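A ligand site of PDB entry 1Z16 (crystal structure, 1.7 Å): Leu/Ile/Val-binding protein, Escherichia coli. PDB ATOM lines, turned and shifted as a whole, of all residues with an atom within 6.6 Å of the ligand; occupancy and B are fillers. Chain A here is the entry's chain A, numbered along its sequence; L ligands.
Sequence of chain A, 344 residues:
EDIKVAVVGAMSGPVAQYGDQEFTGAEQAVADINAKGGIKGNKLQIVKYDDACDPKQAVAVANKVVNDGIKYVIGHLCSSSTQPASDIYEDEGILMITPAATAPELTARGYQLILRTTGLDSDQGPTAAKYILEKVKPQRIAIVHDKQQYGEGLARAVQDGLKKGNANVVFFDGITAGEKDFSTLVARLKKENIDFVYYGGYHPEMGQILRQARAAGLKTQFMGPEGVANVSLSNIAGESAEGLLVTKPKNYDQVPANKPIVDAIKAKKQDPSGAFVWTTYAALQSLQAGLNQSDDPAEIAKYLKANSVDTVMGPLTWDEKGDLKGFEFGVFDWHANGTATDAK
The backbone NH (N) of Ser 79 lies within hydrogen-bond range of an oxygen (O1) of the ligand (2.9 Å). The side-chain hydroxyl (OG) of Ser 79 sits at hydrogen-bond distance from an oxygen (O2) of the ligand (2.6 Å). The side-chain carboxylate of Glu 226 lies within salt-bridge range of a nitrogen (N1) of the ligand. An oxygen (O1) of the ligand sits at hydrogen-bond distance from the side-chain hydroxyl of Tyr 202 (2.7 Å). The backbone carbonyl oxygen of Ala 100 sits at hydrogen-bond distance from a nitrogen (N1) of the ligand (2.9 Å). An oxygen (O2) of the ligand is in hydrogen-bond range of the backbone NH (N) of Thr 102 (2.9 Å). The side-chain hydroxyl of Thr 102 sits at hydrogen-bond distance from a nitrogen (N1) of the ligand (2.9 Å).
The side-chain hydroxyl of Ser 79 lies within hydrogen-bond range of the backbone NH of Thr 102 (3.4 Å). The side-chain hydroxyl (OG) of Ser 79 lies within hydrogen-bond range of the backbone NH (N) of Ala 103 (3.1 Å). The side-chain carboxylate (OE2) of Glu 226 sits at hydrogen-bond distance from the side-chain hydroxyl (OH) of Tyr 150 (2.5 Å). The backbone NH of Glu 226 is in hydrogen-bond range of the side-chain amide oxygen of Gln 124 (2.8 Å). The side-chain carboxylate of Asp 121 is in hydrogen-bond range of the side-chain hydroxyl of Thr 102, 2.6 Å away. N of Gly 227 is in hydrogen-bond range of OH of Tyr 150 (3.0 Å). O of Cys 78 sits at hydrogen-bond distance from OG1 of Thr 82. N of Ala 101 sits at hydrogen-bond distance from O of Leu 77 (3.2 Å).
Merely in contact with the ligand: Tyr 18, Leu 77, Cys 78, Ala 101, Tyr 150, Gly 227 and Phe 276. Hydrophobic or aromatic side chains within 4 Å of the ligand: Tyr 18, Ala 100, Tyr 150, Tyr 202 and Phe 276. Within 4 Å of the ligand: Tyr 18, Leu 77, Cys 78, Ser 79, Ala 100, Ala 101, Thr 102, Tyr 150, Tyr 202, Glu 226, Gly 227 and Phe 276. The nearest printed residue that does not touch the ligand is Ala 103 (4.2 Å).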
ATOM      1  N   VAL A  15       1.075  17.777 -15.809  1.00  0.00           N
ATOM      2  CA  VAL A  15       0.082  18.787 -15.615  1.00  0.00           C
ATOM      3  C   VAL A  15       0.632  20.053 -14.952  1.00  0.00           C
ATOM      4  O   VAL A  15      -0.046  20.775 -14.195  1.00  0.00           O
ATOM      5  CB  VAL A  15      -1.081  18.079 -14.889  1.00  0.00           C
ATOM      6  CG1 VAL A  15      -0.879  18.045 -13.394  1.00  0.00           C
ATOM      7  CG2 VAL A  15      -2.334  18.614 -15.351  1.00  0.00           C
ATOM      8  N   TYR A  18      -0.981  23.678 -14.448  1.00  0.00           N
ATOM      9  CA  TYR A  18      -1.740  24.109 -13.278  1.00  0.00           C
ATOM     10  C   TYR A  18      -0.829  24.846 -12.295  1.00  0.00           C
ATOM     11  O   TYR A  18      -1.206  25.872 -11.736  1.00  0.00           O
ATOM     12  CB  TYR A  18      -2.406  22.928 -12.579  1.00  0.00           C
ATOM     13  CG  TYR A  18      -3.333  22.096 -13.448  1.00  0.00           C
ATOM     14  CD1 TYR A  18      -4.114  22.675 -14.454  1.00  0.00           C
ATOM     15  CD2 TYR A  18      -3.485  20.740 -13.210  1.00  0.00           C
ATOM     16  CE1 TYR A  18      -5.008  21.916 -15.209  1.00  0.00           C
ATOM     17  CE2 TYR A  18      -4.386  19.957 -13.948  1.00  0.00           C
ATOM     18  CZ  TYR A  18      -5.130  20.550 -14.950  1.00  0.00           C
ATOM     19  OH  TYR A  18      -5.958  19.761 -15.681  1.00  0.00           O
ATOM     20  N   CYS A  53       1.310  16.987  -8.716  1.00  0.00           N
ATOM     21  CA  CYS A  53      -0.041  16.392  -8.726  1.00  0.00           C
ATOM     22  C   CYS A  53       0.052  14.876  -8.594  1.00  0.00           C
ATOM     23  O   CYS A  53      -0.746  14.145  -9.178  1.00  0.00           O
ATOM     24  CB  CYS A  53      -0.840  16.765  -9.990  1.00  0.00           C
ATOM     25  SG  CYS A  53      -1.855  18.256  -9.724  1.00  0.00           S
ATOM     26  N   LEU A  77      -3.205  21.293  -5.456  1.00  0.00           N
ATOM     27  CA  LEU A  77      -4.098  21.530  -6.575  1.00  0.00           C
ATOM     28  C   LEU A  77      -5.003  20.385  -6.976  1.00  0.00           C
ATOM     29  O   LEU A  77      -6.196  20.584  -7.084  1.00  0.00           O
ATOM     30  CB  LEU A  77      -3.312  22.025  -7.798  1.00  0.00           C
ATOM     31  CG  LEU A  77      -2.408  23.269  -7.649  1.00  0.00           C
ATOM     32  CD1 LEU A  77      -1.677  23.547  -8.973  1.00  0.00           C
ATOM     33  CD2 LEU A  77      -3.208  24.469  -7.189  1.00  0.00           C
ATOM     34  N   CYS A  78      -4.420  19.241  -7.304  1.00  0.00           N
ATOM     35  CA  CYS A  78      -5.221  18.082  -7.655  1.00  0.00           C
ATOM     36  C   CYS A  78      -5.863  17.454  -6.433  1.00  0.00           C
ATOM     37  O   CYS A  78      -5.260  17.398  -5.371  1.00  0.00           O
ATOM     38  CB  CYS A  78      -4.359  17.046  -8.407  1.00  0.00           C
ATOM     39  SG  CYS A  78      -3.769  17.657 -10.015  1.00  0.00           S
ATOM     40  N   SER A  79      -7.097  16.968  -6.579  1.00  0.00           N
ATOM     41  CA  SER A  79      -7.788  16.395  -5.432  1.00  0.00           C
ATOM     42  C   SER A  79      -7.060  15.188  -4.830  1.00  0.00           C
ATOM     43  O   SER A  79      -6.960  15.073  -3.615  1.00  0.00           O
ATOM     44  CB  SER A  79      -9.224  15.982  -5.822  1.00  0.00           C
ATOM     45  OG  SER A  79     -10.071  17.124  -5.926  1.00  0.00           O
ATOM     46  N   SER A  80      -6.561  14.286  -5.675  1.00  0.00           N
ATOM     47  CA  SER A  80      -5.905  13.100  -5.136  1.00  0.00           C
ATOM     48  C   SER A  80      -4.581  13.415  -4.453  1.00  0.00           C
ATOM     49  O   SER A  80      -4.056  12.593  -3.714  1.00  0.00           O
ATOM     50  CB  SER A  80      -5.723  12.044  -6.234  1.00  0.00           C
ATOM     51  OG  SER A  80      -5.050  12.592  -7.352  1.00  0.00           O
ATOM     52  N   THR A  82      -4.203  16.645  -2.918  1.00  0.00           N
ATOM     53  CA  THR A  82      -4.636  17.507  -1.811  1.00  0.00           C
ATOM     54  C   THR A  82      -5.233  16.720  -0.643  1.00  0.00           C
ATOM     55  O   THR A  82      -4.999  17.035   0.526  1.00  0.00           O
ATOM     56  CB  THR A  82      -5.676  18.543  -2.320  1.00  0.00           C
ATOM     57  OG1 THR A  82      -5.107  19.320  -3.382  1.00  0.00           O
ATOM     58  CG2 THR A  82      -6.089  19.489  -1.206  1.00  0.00           C
ATOM     59  N   ALA A 100      -7.717  25.134  -5.938  1.00  0.00           N
ATOM     60  CA  ALA A 100      -8.161  24.333  -7.092  1.00  0.00           C
ATOM     61  C   ALA A 100      -8.789  22.961  -6.871  1.00  0.00           C
ATOM     62  O   ALA A 100      -9.454  22.472  -7.762  1.00  0.00           O
ATOM     63  CB  ALA A 100      -7.005  24.162  -8.051  1.00  0.00           C
ATOM     64  N   ALA A 101      -8.573  22.328  -5.720  1.00  0.00           N
ATOM     65  CA  ALA A 101      -9.140  20.981  -5.506  1.00  0.00           C
ATOM     66  C   ALA A 101     -10.629  21.080  -5.342  1.00  0.00           C
ATOM     67  O   ALA A 101     -11.125  21.784  -4.460  1.00  0.00           O
ATOM     68  CB  ALA A 101      -8.511  20.326  -4.290  1.00  0.00           C
ATOM     69  N   THR A 102     -11.346  20.319  -6.165  1.00  0.00           N
ATOM     70  CA  THR A 102     -12.809  20.354  -6.206  1.00  0.00           C
ATOM     71  C   THR A 102     -13.605  19.146  -5.715  1.00  0.00           C
ATOM     72  O   THR A 102     -14.839  19.228  -5.620  1.00  0.00           O
ATOM     73  CB  THR A 102     -13.254  20.625  -7.683  1.00  0.00           C
ATOM     74  OG1 THR A 102     -12.614  19.667  -8.524  1.00  0.00           O
ATOM     75  CG2 THR A 102     -12.879  22.046  -8.133  1.00  0.00           C
ATOM     76  N   ALA A 103     -12.938  18.029  -5.390  1.00  0.00           N
ATOM     77  CA  ALA A 103     -13.664  16.844  -4.942  1.00  0.00           C
ATOM     78  C   ALA A 103     -14.331  17.178  -3.627  1.00  0.00           C
ATOM     79  O   ALA A 103     -13.693  17.679  -2.713  1.00  0.00           O
ATOM     80  CB  ALA A 103     -12.697  15.643  -4.791  1.00  0.00           C
ATOM     81  N   LEU A 106     -13.136  16.270   0.345  1.00  0.00           N
ATOM     82  CA  LEU A 106     -12.109  16.988   1.086  1.00  0.00           C
ATOM     83  C   LEU A 106     -12.667  17.762   2.262  1.00  0.00           C
ATOM     84  O   LEU A 106     -12.039  17.830   3.320  1.00  0.00           O
ATOM     85  CB  LEU A 106     -11.335  17.925   0.152  1.00  0.00           C
ATOM     86  CG  LEU A 106     -10.153  17.226  -0.541  1.00  0.00           C
ATOM     87  CD1 LEU A 106     -10.535  15.840  -1.055  1.00  0.00           C
ATOM     88  CD2 LEU A 106      -9.677  18.116  -1.686  1.00  0.00           C
ATOM     89  N   ARG A 116     -11.350  26.427   0.824  1.00  0.00           N
ATOM     90  CA  ARG A 116     -11.089  26.431  -0.613  1.00  0.00           C
ATOM     91  C   ARG A 116     -11.441  27.811  -1.175  1.00  0.00           C
ATOM     92  O   ARG A 116     -12.242  28.548  -0.592  1.00  0.00           O
ATOM     93  CB  ARG A 116     -11.999  25.458  -1.387  1.00  0.00           C
ATOM     94  CG  ARG A 116     -12.244  24.102  -0.785  1.00  0.00           C
ATOM     95  CD  ARG A 116     -12.859  23.138  -1.840  1.00  0.00           C
ATOM     96  NE  ARG A 116     -13.564  22.033  -1.195  1.00  0.00           N
ATOM     97  CZ  ARG A 116     -13.563  20.773  -1.621  1.00  0.00           C
ATOM     98  NH1 ARG A 116     -14.251  19.856  -0.943  1.00  0.00           N
ATOM     99  NH2 ARG A 116     -12.869  20.411  -2.695  1.00  0.00           N
ATOM    100  N   THR A 118     -12.213  27.686  -4.465  1.00  0.00           N
ATOM    101  CA  THR A 118     -12.830  27.242  -5.708  1.00  0.00           C
ATOM    102  C   THR A 118     -14.097  26.512  -5.304  1.00  0.00           C
ATOM    103  O   THR A 118     -14.375  26.384  -4.111  1.00  0.00           O
ATOM    104  CB  THR A 118     -11.911  26.320  -6.560  1.00  0.00           C
ATOM    105  OG1 THR A 118     -12.588  26.064  -7.807  1.00  0.00           O
ATOM    106  CG2 THR A 118     -11.601  25.009  -5.873  1.00  0.00           C
ATOM    107  N   ASP A 121     -17.292  19.763  -6.979  1.00  0.00           N
ATOM    108  CA  ASP A 121     -17.729  18.976  -8.107  1.00  0.00           C
ATOM    109  C   ASP A 121     -19.169  18.478  -7.912  1.00  0.00           C
ATOM    110  O   ASP A 121     -19.808  18.041  -8.862  1.00  0.00           O
ATOM    111  CB  ASP A 121     -16.743  17.844  -8.384  1.00  0.00           C
ATOM    112  CG  ASP A 121     -15.452  18.354  -8.967  1.00  0.00           C
ATOM    113  OD1 ASP A 121     -15.508  19.353  -9.727  1.00  0.00           O
ATOM    114  OD2 ASP A 121     -14.396  17.777  -8.675  1.00  0.00           O
ATOM    115  N   GLN A 124     -20.303  21.272  -9.945  1.00  0.00           N
ATOM    116  CA  GLN A 124     -19.811  21.259 -11.329  1.00  0.00           C
ATOM    117  C   GLN A 124     -20.430  20.124 -12.150  1.00  0.00           C
ATOM    118  O   GLN A 124     -20.834  20.334 -13.313  1.00  0.00           O
ATOM    119  CB  GLN A 124     -18.255  21.177 -11.392  1.00  0.00           C
ATOM    120  CG  GLN A 124     -17.727  21.439 -12.806  1.00  0.00           C
ATOM    121  CD  GLN A 124     -16.196  21.597 -12.969  1.00  0.00           C
ATOM    122  OE1 GLN A 124     -15.737  22.072 -14.002  1.00  0.00           O
ATOM    123  NE2 GLN A 124     -15.409  21.179 -11.957  1.00  0.00           N
ATOM    124  N   GLN A 149      -9.263  10.354  -8.949  1.00  0.00           N
ATOM    125  CA  GLN A 149     -10.289  10.924  -8.088  1.00  0.00           C
ATOM    126  C   GLN A 149     -11.153  12.022  -8.700  1.00  0.00           C
ATOM    127  O   GLN A 149     -12.376  11.923  -8.733  1.00  0.00           O
ATOM    128  CB  GLN A 149      -9.650  11.446  -6.788  1.00  0.00           C
ATOM    129  CG  GLN A 149     -10.686  11.900  -5.745  1.00  0.00           C
ATOM    130  CD  GLN A 149     -10.054  12.252  -4.409  1.00  0.00           C
ATOM    131  OE1 GLN A 149     -10.740  12.718  -3.477  1.00  0.00           O
ATOM    132  NE2 GLN A 149      -8.750  12.032  -4.296  1.00  0.00           N
ATOM    133  N   TYR A 150     -10.512  13.074  -9.207  1.00  0.00           N
ATOM    134  CA  TYR A 150     -11.246  14.174  -9.808  1.00  0.00           C
ATOM    135  C   TYR A 150     -12.119  13.751 -10.994  1.00  0.00           C
ATOM    136  O   TYR A 150     -13.334  13.957 -10.984  1.00  0.00           O
ATOM    137  CB  TYR A 150     -10.249  15.230 -10.282  1.00  0.00           C
ATOM    138  CG  TYR A 150     -10.809  16.304 -11.183  1.00  0.00           C
ATOM    139  CD1 TYR A 150     -11.636  17.304 -10.666  1.00  0.00           C
ATOM    140  CD2 TYR A 150     -10.420  16.376 -12.504  1.00  0.00           C
ATOM    141  CE1 TYR A 150     -12.032  18.374 -11.469  1.00  0.00           C
ATOM    142  CE2 TYR A 150     -10.813  17.459 -13.326  1.00  0.00           C
ATOM    143  CZ  TYR A 150     -11.610  18.449 -12.788  1.00  0.00           C
ATOM    144  OH  TYR A 150     -11.940  19.543 -13.539  1.00  0.00           O
ATOM    145  N   GLY A 151     -11.486  13.150 -11.992  1.00  0.00           N
ATOM    146  CA  GLY A 151     -12.195  12.770 -13.199  1.00  0.00           C
ATOM    147  C   GLY A 151     -13.298  11.743 -13.028  1.00  0.00           C
ATOM    148  O   GLY A 151     -14.382  11.913 -13.593  1.00  0.00           O
ATOM    149  N   LEU A 154     -16.345  13.306 -11.109  1.00  0.00           N
ATOM    150  CA  LEU A 154     -17.217  14.084 -12.001  1.00  0.00           C
ATOM    151  C   LEU A 154     -18.004  13.188 -12.977  1.00  0.00           C
ATOM    152  O   LEU A 154     -19.203  13.422 -13.208  1.00  0.00           O
ATOM    153  CB  LEU A 154     -16.390  15.087 -12.822  1.00  0.00           C
ATOM    154  CG  LEU A 154     -16.065  16.386 -12.047  1.00  0.00           C
ATOM    155  CD1 LEU A 154     -14.910  17.147 -12.694  1.00  0.00           C
ATOM    156  CD2 LEU A 154     -17.336  17.272 -11.981  1.00  0.00           C
ATOM    157  N   GLY A 201     -11.564  14.515 -16.471  1.00  0.00           N
ATOM    158  CA  GLY A 201     -10.128  14.360 -16.323  1.00  0.00           C
ATOM    159  C   GLY A 201      -9.401  15.666 -16.616  1.00  0.00           C
ATOM    160  O   GLY A 201     -10.002  16.754 -16.580  1.00  0.00           O
ATOM    161  N   TYR A 202      -8.118  15.553 -16.928  1.00  0.00           N
ATOM    162  CA  TYR A 202      -7.265  16.702 -17.192  1.00  0.00           C
ATOM    163  C   TYR A 202      -6.938  16.897 -18.681  1.00  0.00           C
ATOM    164  O   TYR A 202      -7.185  16.022 -19.519  1.00  0.00           O
ATOM    165  CB  TYR A 202      -5.979  16.570 -16.363  1.00  0.00           C
ATOM    166  CG  TYR A 202      -6.216  16.386 -14.869  1.00  0.00           C
ATOM    167  CD1 TYR A 202      -7.055  17.258 -14.151  1.00  0.00           C
ATOM    168  CD2 TYR A 202      -5.584  15.369 -14.169  1.00  0.00           C
ATOM    169  CE1 TYR A 202      -7.243  17.110 -12.748  1.00  0.00           C
ATOM    170  CE2 TYR A 202      -5.771  15.217 -12.753  1.00  0.00           C
ATOM    171  CZ  TYR A 202      -6.591  16.089 -12.064  1.00  0.00           C
ATOM    172  OH  TYR A 202      -6.715  15.973 -10.695  1.00  0.00           O
ATOM    173  N   GLU A 226     -13.493  22.017 -15.615  1.00  0.00           N
ATOM    174  CA  GLU A 226     -12.524  23.115 -15.626  1.00  0.00           C
ATOM    175  C   GLU A 226     -11.069  22.696 -15.829  1.00  0.00           C
ATOM    176  O   GLU A 226     -10.252  23.493 -16.302  1.00  0.00           O
ATOM    177  CB  GLU A 226     -12.732  24.013 -14.364  1.00  0.00           C
ATOM    178  CG  GLU A 226     -11.686  23.901 -13.237  1.00  0.00           C
ATOM    179  CD  GLU A 226     -11.753  22.617 -12.430  1.00  0.00           C
ATOM    180  OE1 GLU A 226     -10.886  22.440 -11.559  1.00  0.00           O
ATOM    181  OE2 GLU A 226     -12.653  21.775 -12.658  1.00  0.00           O
ATOM    182  N   GLY A 227     -10.756  21.433 -15.531  1.00  0.00           N
ATOM    183  CA  GLY A 227      -9.405  20.930 -15.708  1.00  0.00           C
ATOM    184  C   GLY A 227      -8.929  20.852 -17.146  1.00  0.00           C
ATOM    185  O   GLY A 227      -7.736  20.686 -17.395  1.00  0.00           O
ATOM    186  N   VAL A 228      -9.843  20.947 -18.113  1.00  0.00           N
ATOM    187  CA  VAL A 228      -9.389  20.889 -19.509  1.00  0.00           C
ATOM    188  C   VAL A 228      -9.463  22.256 -20.161  1.00  0.00           C
ATOM    189  O   VAL A 228      -9.043  22.412 -21.313  1.00  0.00           O
ATOM    190  CB  VAL A 228     -10.225  19.900 -20.387  1.00  0.00           C
ATOM    191  CG1 VAL A 228     -10.274  18.516 -19.729  1.00  0.00           C
ATOM    192  CG2 VAL A 228     -11.634  20.467 -20.626  1.00  0.00           C
ATOM    193  N   PHE A 276      -6.810  29.528 -12.378  1.00  0.00           N
ATOM    194  CA  PHE A 276      -6.072  29.370 -11.133  1.00  0.00           C
ATOM    195  C   PHE A 276      -5.185  30.526 -10.745  1.00  0.00           C
ATOM    196  O   PHE A 276      -4.686  30.612  -9.627  1.00  0.00           O
ATOM    197  CB  PHE A 276      -5.337  28.034 -11.163  1.00  0.00           C
ATOM    198  CG  PHE A 276      -6.252  26.879 -11.487  1.00  0.00           C
ATOM    199  CD1 PHE A 276      -7.483  26.753 -10.825  1.00  0.00           C
ATOM    200  CD2 PHE A 276      -5.929  25.957 -12.474  1.00  0.00           C
ATOM    201  CE1 PHE A 276      -8.384  25.751 -11.153  1.00  0.00           C
ATOM    202  CE2 PHE A 276      -6.828  24.934 -12.814  1.00  0.00           C
ATOM    203  CZ  PHE A 276      -8.056  24.845 -12.150  1.00  0.00           C
HETATM  204  N1  LIG L   1     -10.176  20.581  -9.839  1.00  0.00           N
HETATM  205  C1  LIG L   1      -9.082  19.593 -10.083  1.00  0.00           C
HETATM  206  C2  LIG L   1      -9.033  18.544  -8.978  1.00  0.00           C
HETATM  207  O1  LIG L   1      -8.247  17.574  -9.138  1.00  0.00           O
HETATM  208  C3  LIG L   1      -7.705  20.305 -10.166  1.00  0.00           C
HETATM  209  C4  LIG L   1      -7.510  21.447 -11.152  1.00  0.00           C
HETATM  210  C5  LIG L   1      -6.044  21.935 -11.057  1.00  0.00           C
HETATM  211  C6  LIG L   1      -7.808  21.002 -12.561  1.00  0.00           C
HETATM  212  O2  LIG L   1      -9.758  18.687  -7.976  1.00  0.00           O
